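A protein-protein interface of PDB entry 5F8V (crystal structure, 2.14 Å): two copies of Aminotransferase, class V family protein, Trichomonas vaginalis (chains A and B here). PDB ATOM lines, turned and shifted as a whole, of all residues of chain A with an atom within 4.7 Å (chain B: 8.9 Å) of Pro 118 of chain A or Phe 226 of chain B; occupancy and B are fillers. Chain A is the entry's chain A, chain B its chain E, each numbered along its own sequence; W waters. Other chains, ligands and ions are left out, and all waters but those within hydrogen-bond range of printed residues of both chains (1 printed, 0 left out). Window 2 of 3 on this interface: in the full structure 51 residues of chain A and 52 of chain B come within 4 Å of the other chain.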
ATOM      1  N   PHE A  87       2.469   2.146 -19.746  1.00  0.00           N
ATOM      2  CA  PHE A  87       2.403   2.242 -21.216  1.00  0.00           C
ATOM      3  C   PHE A  87       2.487   3.695 -21.677  1.00  0.00           C
ATOM      4  O   PHE A  87       3.245   4.005 -22.598  1.00  0.00           O
ATOM      5  CB  PHE A  87       1.116   1.632 -21.788  1.00  0.00           C
ATOM      6  CG  PHE A  87       1.193   0.162 -22.034  1.00  0.00           C
ATOM      7  CD1 PHE A  87       2.030  -0.347 -23.030  1.00  0.00           C
ATOM      8  CD2 PHE A  87       0.424  -0.730 -21.283  1.00  0.00           C
ATOM      9  CE1 PHE A  87       2.108  -1.706 -23.255  1.00  0.00           C
ATOM     10  CE2 PHE A  87       0.500  -2.093 -21.514  1.00  0.00           C
ATOM     11  CZ  PHE A  87       1.341  -2.581 -22.504  1.00  0.00           C
ATOM     12  N   LEU A 115       4.495  -6.385 -16.124  1.00  0.00           N
ATOM     13  CA  LEU A 115       4.613  -6.000 -17.534  1.00  0.00           C
ATOM     14  C   LEU A 115       6.071  -5.986 -18.026  1.00  0.00           C
ATOM     15  O   LEU A 115       6.324  -6.302 -19.182  1.00  0.00           O
ATOM     16  CB  LEU A 115       3.957  -4.639 -17.791  1.00  0.00           C
ATOM     17  CG  LEU A 115       2.428  -4.570 -17.677  1.00  0.00           C
ATOM     18  CD1 LEU A 115       1.973  -3.121 -17.646  1.00  0.00           C
ATOM     19  CD2 LEU A 115       1.732  -5.322 -18.800  1.00  0.00           C
ATOM     20  N   ALA A 116       7.004  -5.606 -17.150  1.00  0.00           N
ATOM     21  CA  ALA A 116       8.447  -5.713 -17.394  1.00  0.00           C
ATOM     22  C   ALA A 116       8.890  -5.026 -18.687  1.00  0.00           C
ATOM     23  O   ALA A 116       9.337  -5.680 -19.625  1.00  0.00           O
ATOM     24  CB  ALA A 116       8.885  -7.180 -17.380  1.00  0.00           C
ATOM     25  N   PHE A 117       8.749  -3.705 -18.733  1.00  0.00           N
ATOM     26  CA  PHE A 117       9.208  -2.935 -19.884  1.00  0.00           C
ATOM     27  C   PHE A 117      10.743  -2.945 -19.889  1.00  0.00           C
ATOM     28  O   PHE A 117      11.342  -2.516 -18.911  1.00  0.00           O
ATOM     29  CB  PHE A 117       8.654  -1.508 -19.845  1.00  0.00           C
ATOM     30  CG  PHE A 117       7.177  -1.426 -20.133  1.00  0.00           C
ATOM     31  CD1 PHE A 117       6.250  -1.319 -19.096  1.00  0.00           C
ATOM     32  CD2 PHE A 117       6.707  -1.463 -21.441  1.00  0.00           C
ATOM     33  CE1 PHE A 117       4.887  -1.243 -19.360  1.00  0.00           C
ATOM     34  CE2 PHE A 117       5.340  -1.391 -21.711  1.00  0.00           C
ATOM     35  CZ  PHE A 117       4.432  -1.273 -20.665  1.00  0.00           C
ATOM     36  N   PRO A 118      11.379  -3.476 -20.963  1.00  0.00           N
ATOM     37  CA  PRO A 118      12.844  -3.578 -20.996  1.00  0.00           C
ATOM     38  C   PRO A 118      13.538  -2.269 -20.645  1.00  0.00           C
ATOM     39  O   PRO A 118      13.136  -1.205 -21.133  1.00  0.00           O
ATOM     40  CB  PRO A 118      13.133  -3.953 -22.455  1.00  0.00           C
ATOM     41  CG  PRO A 118      11.950  -4.746 -22.858  1.00  0.00           C
ATOM     42  CD  PRO A 118      10.783  -4.079 -22.173  1.00  0.00           C
ATOM     43  N   GLY A 119      14.539  -2.354 -19.772  1.00  0.00           N
ATOM     44  CA  GLY A 119      15.368  -1.209 -19.414  1.00  0.00           C
ATOM     45  C   GLY A 119      14.748  -0.230 -18.436  1.00  0.00           C
ATOM     46  O   GLY A 119      15.242   0.887 -18.306  1.00  0.00           O
ATOM     47  N   VAL A 120      13.672  -0.630 -17.751  1.00  0.00           N
ATOM     48  CA  VAL A 120      13.013   0.239 -16.779  1.00  0.00           C
ATOM     49  C   VAL A 120      13.086  -0.397 -15.402  1.00  0.00           C
ATOM     50  O   VAL A 120      12.590  -1.508 -15.202  1.00  0.00           O
ATOM     51  CB  VAL A 120      11.541   0.534 -17.138  1.00  0.00           C
ATOM     52  CG1 VAL A 120      10.935   1.506 -16.139  1.00  0.00           C
ATOM     53  CG2 VAL A 120      11.433   1.107 -18.551  1.00  0.00           C
ATOM     54  N   PHE A 226       3.203  -2.103 -27.973  1.00  0.00           N
ATOM     55  CA  PHE A 226       2.148  -3.054 -27.588  1.00  0.00           C
ATOM     56  C   PHE A 226       1.049  -2.456 -26.705  1.00  0.00           C
ATOM     57  O   PHE A 226       0.297  -3.199 -26.079  1.00  0.00           O
ATOM     58  CB  PHE A 226       2.728  -4.337 -26.956  1.00  0.00           C
ATOM     59  CG  PHE A 226       3.908  -4.892 -27.704  1.00  0.00           C
ATOM     60  CD1 PHE A 226       3.729  -5.558 -28.910  1.00  0.00           C
ATOM     61  CD2 PHE A 226       5.198  -4.733 -27.213  1.00  0.00           C
ATOM     62  CE1 PHE A 226       4.813  -6.063 -29.609  1.00  0.00           C
ATOM     63  CE2 PHE A 226       6.295  -5.235 -27.910  1.00  0.00           C
ATOM     64  CZ  PHE A 226       6.100  -5.902 -29.110  1.00  0.00           C
ATOM     65  N   SER B  83      -7.783  -5.670 -29.551  1.00  0.00           N
ATOM     66  CA  SER B  83      -6.432  -5.724 -29.005  1.00  0.00           C
ATOM     67  C   SER B  83      -6.203  -7.026 -28.247  1.00  0.00           C
ATOM     68  O   SER B  83      -5.198  -7.700 -28.466  1.00  0.00           O
ATOM     69  CB  SER B  83      -6.174  -4.540 -28.061  1.00  0.00           C
ATOM     70  OG  SER B  83      -6.520  -3.310 -28.671  1.00  0.00           O
ATOM     71  N   PHE B  87      -3.268 -10.783 -28.411  1.00  0.00           N
ATOM     72  CA  PHE B  87      -2.558 -11.032 -27.137  1.00  0.00           C
ATOM     73  C   PHE B  87      -2.856 -12.412 -26.558  1.00  0.00           C
ATOM     74  O   PHE B  87      -1.985 -13.048 -25.989  1.00  0.00           O
ATOM     75  CB  PHE B  87      -2.942 -10.003 -26.058  1.00  0.00           C
ATOM     76  CG  PHE B  87      -2.126  -8.745 -26.075  1.00  0.00           C
ATOM     77  CD1 PHE B  87      -0.802  -8.757 -25.672  1.00  0.00           C
ATOM     78  CD2 PHE B  87      -2.697  -7.532 -26.445  1.00  0.00           C
ATOM     79  CE1 PHE B  87      -0.053  -7.585 -25.657  1.00  0.00           C
ATOM     80  CE2 PHE B  87      -1.957  -6.359 -26.435  1.00  0.00           C
ATOM     81  CZ  PHE B  87      -0.627  -6.388 -26.047  1.00  0.00           C
ATOM     82  N   LEU B 115      -0.082  -3.293 -33.494  1.00  0.00           N
ATOM     83  CA  LEU B 115       0.542  -3.869 -32.293  1.00  0.00           C
ATOM     84  C   LEU B 115       1.870  -4.563 -32.625  1.00  0.00           C
ATOM     85  O   LEU B 115       2.788  -4.558 -31.805  1.00  0.00           O
ATOM     86  CB  LEU B 115      -0.405  -4.849 -31.594  1.00  0.00           C
ATOM     87  CG  LEU B 115      -1.576  -4.226 -30.826  1.00  0.00           C
ATOM     88  CD1 LEU B 115      -2.675  -5.253 -30.615  1.00  0.00           C
ATOM     89  CD2 LEU B 115      -1.123  -3.640 -29.499  1.00  0.00           C
ATOM     90  N   ALA B 116       1.953  -5.161 -33.820  1.00  0.00           N
ATOM     91  CA  ALA B 116       3.218  -5.658 -34.388  1.00  0.00           C
ATOM     92  C   ALA B 116       3.955  -6.631 -33.472  1.00  0.00           C
ATOM     93  O   ALA B 116       5.095  -6.384 -33.083  1.00  0.00           O
ATOM     94  CB  ALA B 116       4.125  -4.490 -34.766  1.00  0.00           C
ATOM     95  N   PHE B 117       3.291  -7.728 -33.118  1.00  0.00           N
ATOM     96  CA  PHE B 117       3.933  -8.792 -32.349  1.00  0.00           C
ATOM     97  C   PHE B 117       5.055  -9.414 -33.209  1.00  0.00           C
ATOM     98  O   PHE B 117       4.787  -9.810 -34.344  1.00  0.00           O
ATOM     99  CB  PHE B 117       2.913  -9.850 -31.933  1.00  0.00           C
ATOM    100  CG  PHE B 117       1.889  -9.350 -30.942  1.00  0.00           C
ATOM    101  CD1 PHE B 117       2.259  -9.049 -29.636  1.00  0.00           C
ATOM    102  CD2 PHE B 117       0.557  -9.180 -31.312  1.00  0.00           C
ATOM    103  CE1 PHE B 117       1.326  -8.584 -28.717  1.00  0.00           C
ATOM    104  CE2 PHE B 117      -0.382  -8.719 -30.393  1.00  0.00           C
ATOM    105  CZ  PHE B 117       0.002  -8.419 -29.096  1.00  0.00           C
ATOM    106  N   PRO B 118       6.311  -9.457 -32.693  1.00  0.00           N
ATOM    107  CA  PRO B 118       7.460  -9.989 -33.453  1.00  0.00           C
ATOM    108  C   PRO B 118       7.261 -11.387 -34.040  1.00  0.00           C
ATOM    109  O   PRO B 118       6.722 -12.266 -33.374  1.00  0.00           O
ATOM    110  CB  PRO B 118       8.582 -10.029 -32.409  1.00  0.00           C
ATOM    111  CG  PRO B 118       8.253  -8.926 -31.471  1.00  0.00           C
ATOM    112  CD  PRO B 118       6.751  -8.855 -31.417  1.00  0.00           C
ATOM    113  N   VAL B 223      -0.155 -16.487 -23.408  1.00  0.00           N
ATOM    114  CA  VAL B 223      -0.405 -15.061 -23.639  1.00  0.00           C
ATOM    115  C   VAL B 223       0.884 -14.383 -24.129  1.00  0.00           C
ATOM    116  O   VAL B 223       1.971 -14.708 -23.660  1.00  0.00           O
ATOM    117  CB  VAL B 223      -0.960 -14.363 -22.360  1.00  0.00           C
ATOM    118  CG1 VAL B 223       0.111 -14.196 -21.284  1.00  0.00           C
ATOM    119  CG2 VAL B 223      -1.585 -13.014 -22.693  1.00  0.00           C
ATOM    120  N   LYS B 224       0.757 -13.465 -25.085  1.00  0.00           N
ATOM    121  CA  LYS B 224       1.892 -12.662 -25.555  1.00  0.00           C
ATOM    122  C   LYS B 224       2.395 -11.730 -24.452  1.00  0.00           C
ATOM    123  O   LYS B 224       1.624 -11.375 -23.563  1.00  0.00           O
ATOM    124  CB  LYS B 224       1.499 -11.815 -26.777  1.00  0.00           C
ATOM    125  CG  LYS B 224       1.357 -12.594 -28.074  1.00  0.00           C
ATOM    126  CD  LYS B 224       2.715 -12.995 -28.633  1.00  0.00           C
ATOM    127  CE  LYS B 224       2.557 -13.816 -29.897  1.00  0.00           C
ATOM    128  NZ  LYS B 224       3.877 -14.286 -30.402  1.00  0.00           N
ATOM    129  N   PRO B 225       3.677 -11.309 -24.514  1.00  0.00           N
ATOM    130  CA  PRO B 225       4.171 -10.359 -23.495  1.00  0.00           C
ATOM    131  C   PRO B 225       3.489  -8.982 -23.540  1.00  0.00           C
ATOM    132  O   PRO B 225       2.905  -8.612 -24.562  1.00  0.00           O
ATOM    133  CB  PRO B 225       5.674 -10.227 -23.812  1.00  0.00           C
ATOM    134  CG  PRO B 225       5.998 -11.339 -24.763  1.00  0.00           C
ATOM    135  CD  PRO B 225       4.728 -11.667 -25.487  1.00  0.00           C
ATOM    136  N   PHE B 226       3.569  -8.260 -22.420  1.00  0.00           N
ATOM    137  CA  PHE B 226       2.963  -6.924 -22.226  1.00  0.00           C
ATOM    138  C   PHE B 226       1.438  -6.885 -22.294  1.00  0.00           C
ATOM    139  O   PHE B 226       0.860  -5.830 -22.519  1.00  0.00           O
ATOM    140  CB  PHE B 226       3.537  -5.871 -23.199  1.00  0.00           C
ATOM    141  CG  PHE B 226       5.032  -5.846 -23.260  1.00  0.00           C
ATOM    142  CD1 PHE B 226       5.769  -5.223 -22.266  1.00  0.00           C
ATOM    143  CD2 PHE B 226       5.710  -6.449 -24.323  1.00  0.00           C
ATOM    144  CE1 PHE B 226       7.153  -5.206 -22.325  1.00  0.00           C
ATOM    145  CE2 PHE B 226       7.095  -6.436 -24.385  1.00  0.00           C
ATOM    146  CZ  PHE B 226       7.819  -5.814 -23.384  1.00  0.00           C
ATOM    147  N   CYS B 227       0.774  -8.018 -22.099  1.00  0.00           N
ATOM    148  CA  CYS B 227      -0.680  -8.027 -22.051  1.00  0.00           C
ATOM    149  C   CYS B 227      -1.125  -7.461 -20.699  1.00  0.00           C
ATOM    150  O   CYS B 227      -0.675  -7.957 -19.674  1.00  0.00           O
ATOM    151  CB  CYS B 227      -1.198  -9.445 -22.215  1.00  0.00           C
ATOM    152  SG  CYS B 227      -2.986  -9.545 -22.293  1.00  0.00           S
ATOM    153  N   PRO B 228      -1.981  -6.408 -20.686  1.00  0.00           N
ATOM    154  CA  PRO B 228      -2.559  -5.942 -19.427  1.00  0.00           C
ATOM    155  C   PRO B 228      -3.254  -7.094 -18.707  1.00  0.00           C
ATOM    156  O   PRO B 228      -3.984  -7.866 -19.354  1.00  0.00           O
ATOM    157  CB  PRO B 228      -3.573  -4.886 -19.878  1.00  0.00           C
ATOM    158  CG  PRO B 228      -2.993  -4.361 -21.136  1.00  0.00           C
ATOM    159  CD  PRO B 228      -2.426  -5.570 -21.812  1.00  0.00           C
ATOM    160  N   ILE B 229      -3.013  -7.229 -17.401  1.00  0.00           N
ATOM    161  CA  ILE B 229      -3.467  -8.434 -16.678  1.00  0.00           C
ATOM    162  C   ILE B 229      -4.970  -8.699 -16.831  1.00  0.00           C
ATOM    163  O   ILE B 229      -5.371  -9.846 -17.060  1.00  0.00           O
ATOM    164  CB  ILE B 229      -3.024  -8.480 -15.189  1.00  0.00           C
ATOM    165  CG1 ILE B 229      -3.376  -9.844 -14.566  1.00  0.00           C
ATOM    166  CG2 ILE B 229      -3.639  -7.344 -14.372  1.00  0.00           C
ATOM    167  CD1 ILE B 229      -2.564 -10.197 -13.344  1.00  0.00           C
ATOM    168  N   MET B 231      -6.894  -7.966 -19.350  1.00  0.00           N
ATOM    169  CA  MET B 231      -7.195  -8.413 -20.730  1.00  0.00           C
ATOM    170  C   MET B 231      -6.685  -9.833 -21.046  1.00  0.00           C
ATOM    171  O   MET B 231      -6.858 -10.333 -22.172  1.00  0.00           O
ATOM    172  CB  MET B 231      -6.619  -7.422 -21.746  1.00  0.00           C
ATOM    173  CG  MET B 231      -7.276  -6.051 -21.716  1.00  0.00           C
ATOM    174  SD  MET B 231      -6.356  -4.841 -22.680  1.00  0.00           S
ATOM    175  CE  MET B 231      -6.393  -5.593 -24.308  1.00  0.00           C
ATOM    176  N   ASP B 232      -6.046 -10.472 -20.069  1.00  0.00           N
ATOM    177  CA  ASP B 232      -5.682 -11.873 -20.158  1.00  0.00           C
ATOM    178  C   ASP B 232      -6.941 -12.675 -19.813  1.00  0.00           C
ATOM    179  O   ASP B 232      -7.348 -12.719 -18.659  1.00  0.00           O
ATOM    180  CB  ASP B 232      -4.529 -12.169 -19.191  1.00  0.00           C
ATOM    181  CG  ASP B 232      -4.011 -13.593 -19.297  1.00  0.00           C
ATOM    182  OD1 ASP B 232      -4.738 -14.463 -19.818  1.00  0.00           O
ATOM    183  OD2 ASP B 232      -2.873 -13.836 -18.843  1.00  0.00           O
HETATM  184  O   HOH W   1       5.342  -8.713 -20.288  1.00  0.00           O
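Gly 119 of chain A touches none of the printed residues of chain B. Printed residues of chain A within 4 Å of Phe 87 of chain B: Phe 226 (3.3 Å). Of the printed residues of chain A, Ala 116 of chain B touches Phe 226. Printed residues of chain A within 4 Å of Pro 118 of chain B: Phe 226. Phe 226 of chain B touches six residues of chain A. Printed residues of chain A within 4 Å of Cys 227 of chain B: Leu 115 (3.7 Å). Met 231 of chain B touches none of the printed residues of chain A. The nearest printed residue of chain A that does not touch Phe 226 of chain B is Gly 119 of chain A (8.3 Å).
Among the printed residues, merely in contact across the chains: Phe 226 of chain A with Leu 115 of chain B, Phe 87 of chain A with Phe 226 of chain B, Leu 115 of chain A with Phe 226 of chain B, Phe 226 of chain A with Phe 87 of chain B, Phe 226 of chain A with Phe 226 of chain B, Phe 226 of chain A with Ala 116 of chain B, Ala 116 of chain A with Phe 226 of chain B, Pro 118 of chain A with Phe 226 of chain B, Leu 115 of chain A with Cys 227 of chain B, Phe 226 of chain A with Pro 118 of chain B, Phe 226 of chain A with Phe 117 of chain B and Phe 117 of chain A with Phe 226 of chain B.
Water W1 lies within hydrogen-bond range of the backbone NH of Phe 226 of chain B and the backbone carbonyl oxygen of Leu 115 of chain A.
The backbone NH (N) of Lys 224 of chain B lies within hydrogen-bond range of the backbone carbonyl oxygen (O) of Phe 87 of chain B, at 2.9 Å.
Printed residues of chain A that touch a printed residue of chain B: Phe 87, Leu 115, Ala 116, Phe 117, Pro 118 and Phe 226. Among the printed residues, no Asp or Glu carboxylate lies within 4 Å of a Lys or Arg side-chain nitrogen of the other chain.
Leu 115 of chain A touches Phe 226 of chain B, and with the chains exchanged Phe 226 of chain A touches Leu 115 of chain B. Ala 116 of chain A touches Phe 226 of chain B, and with the chains exchanged Phe 226 of chain A touches Ala 116 of chain B. Phe 117 of chain A touches Phe 226 of chain B, and with the chains exchanged Phe 226 of chain A touches Phe 117 of chain B. Pro 118 of chain A touches Phe 226 of chain B, and with the chains exchanged Phe 226 of chain A touches Pro 118 of chain B. 6 positions are printed for both chains.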
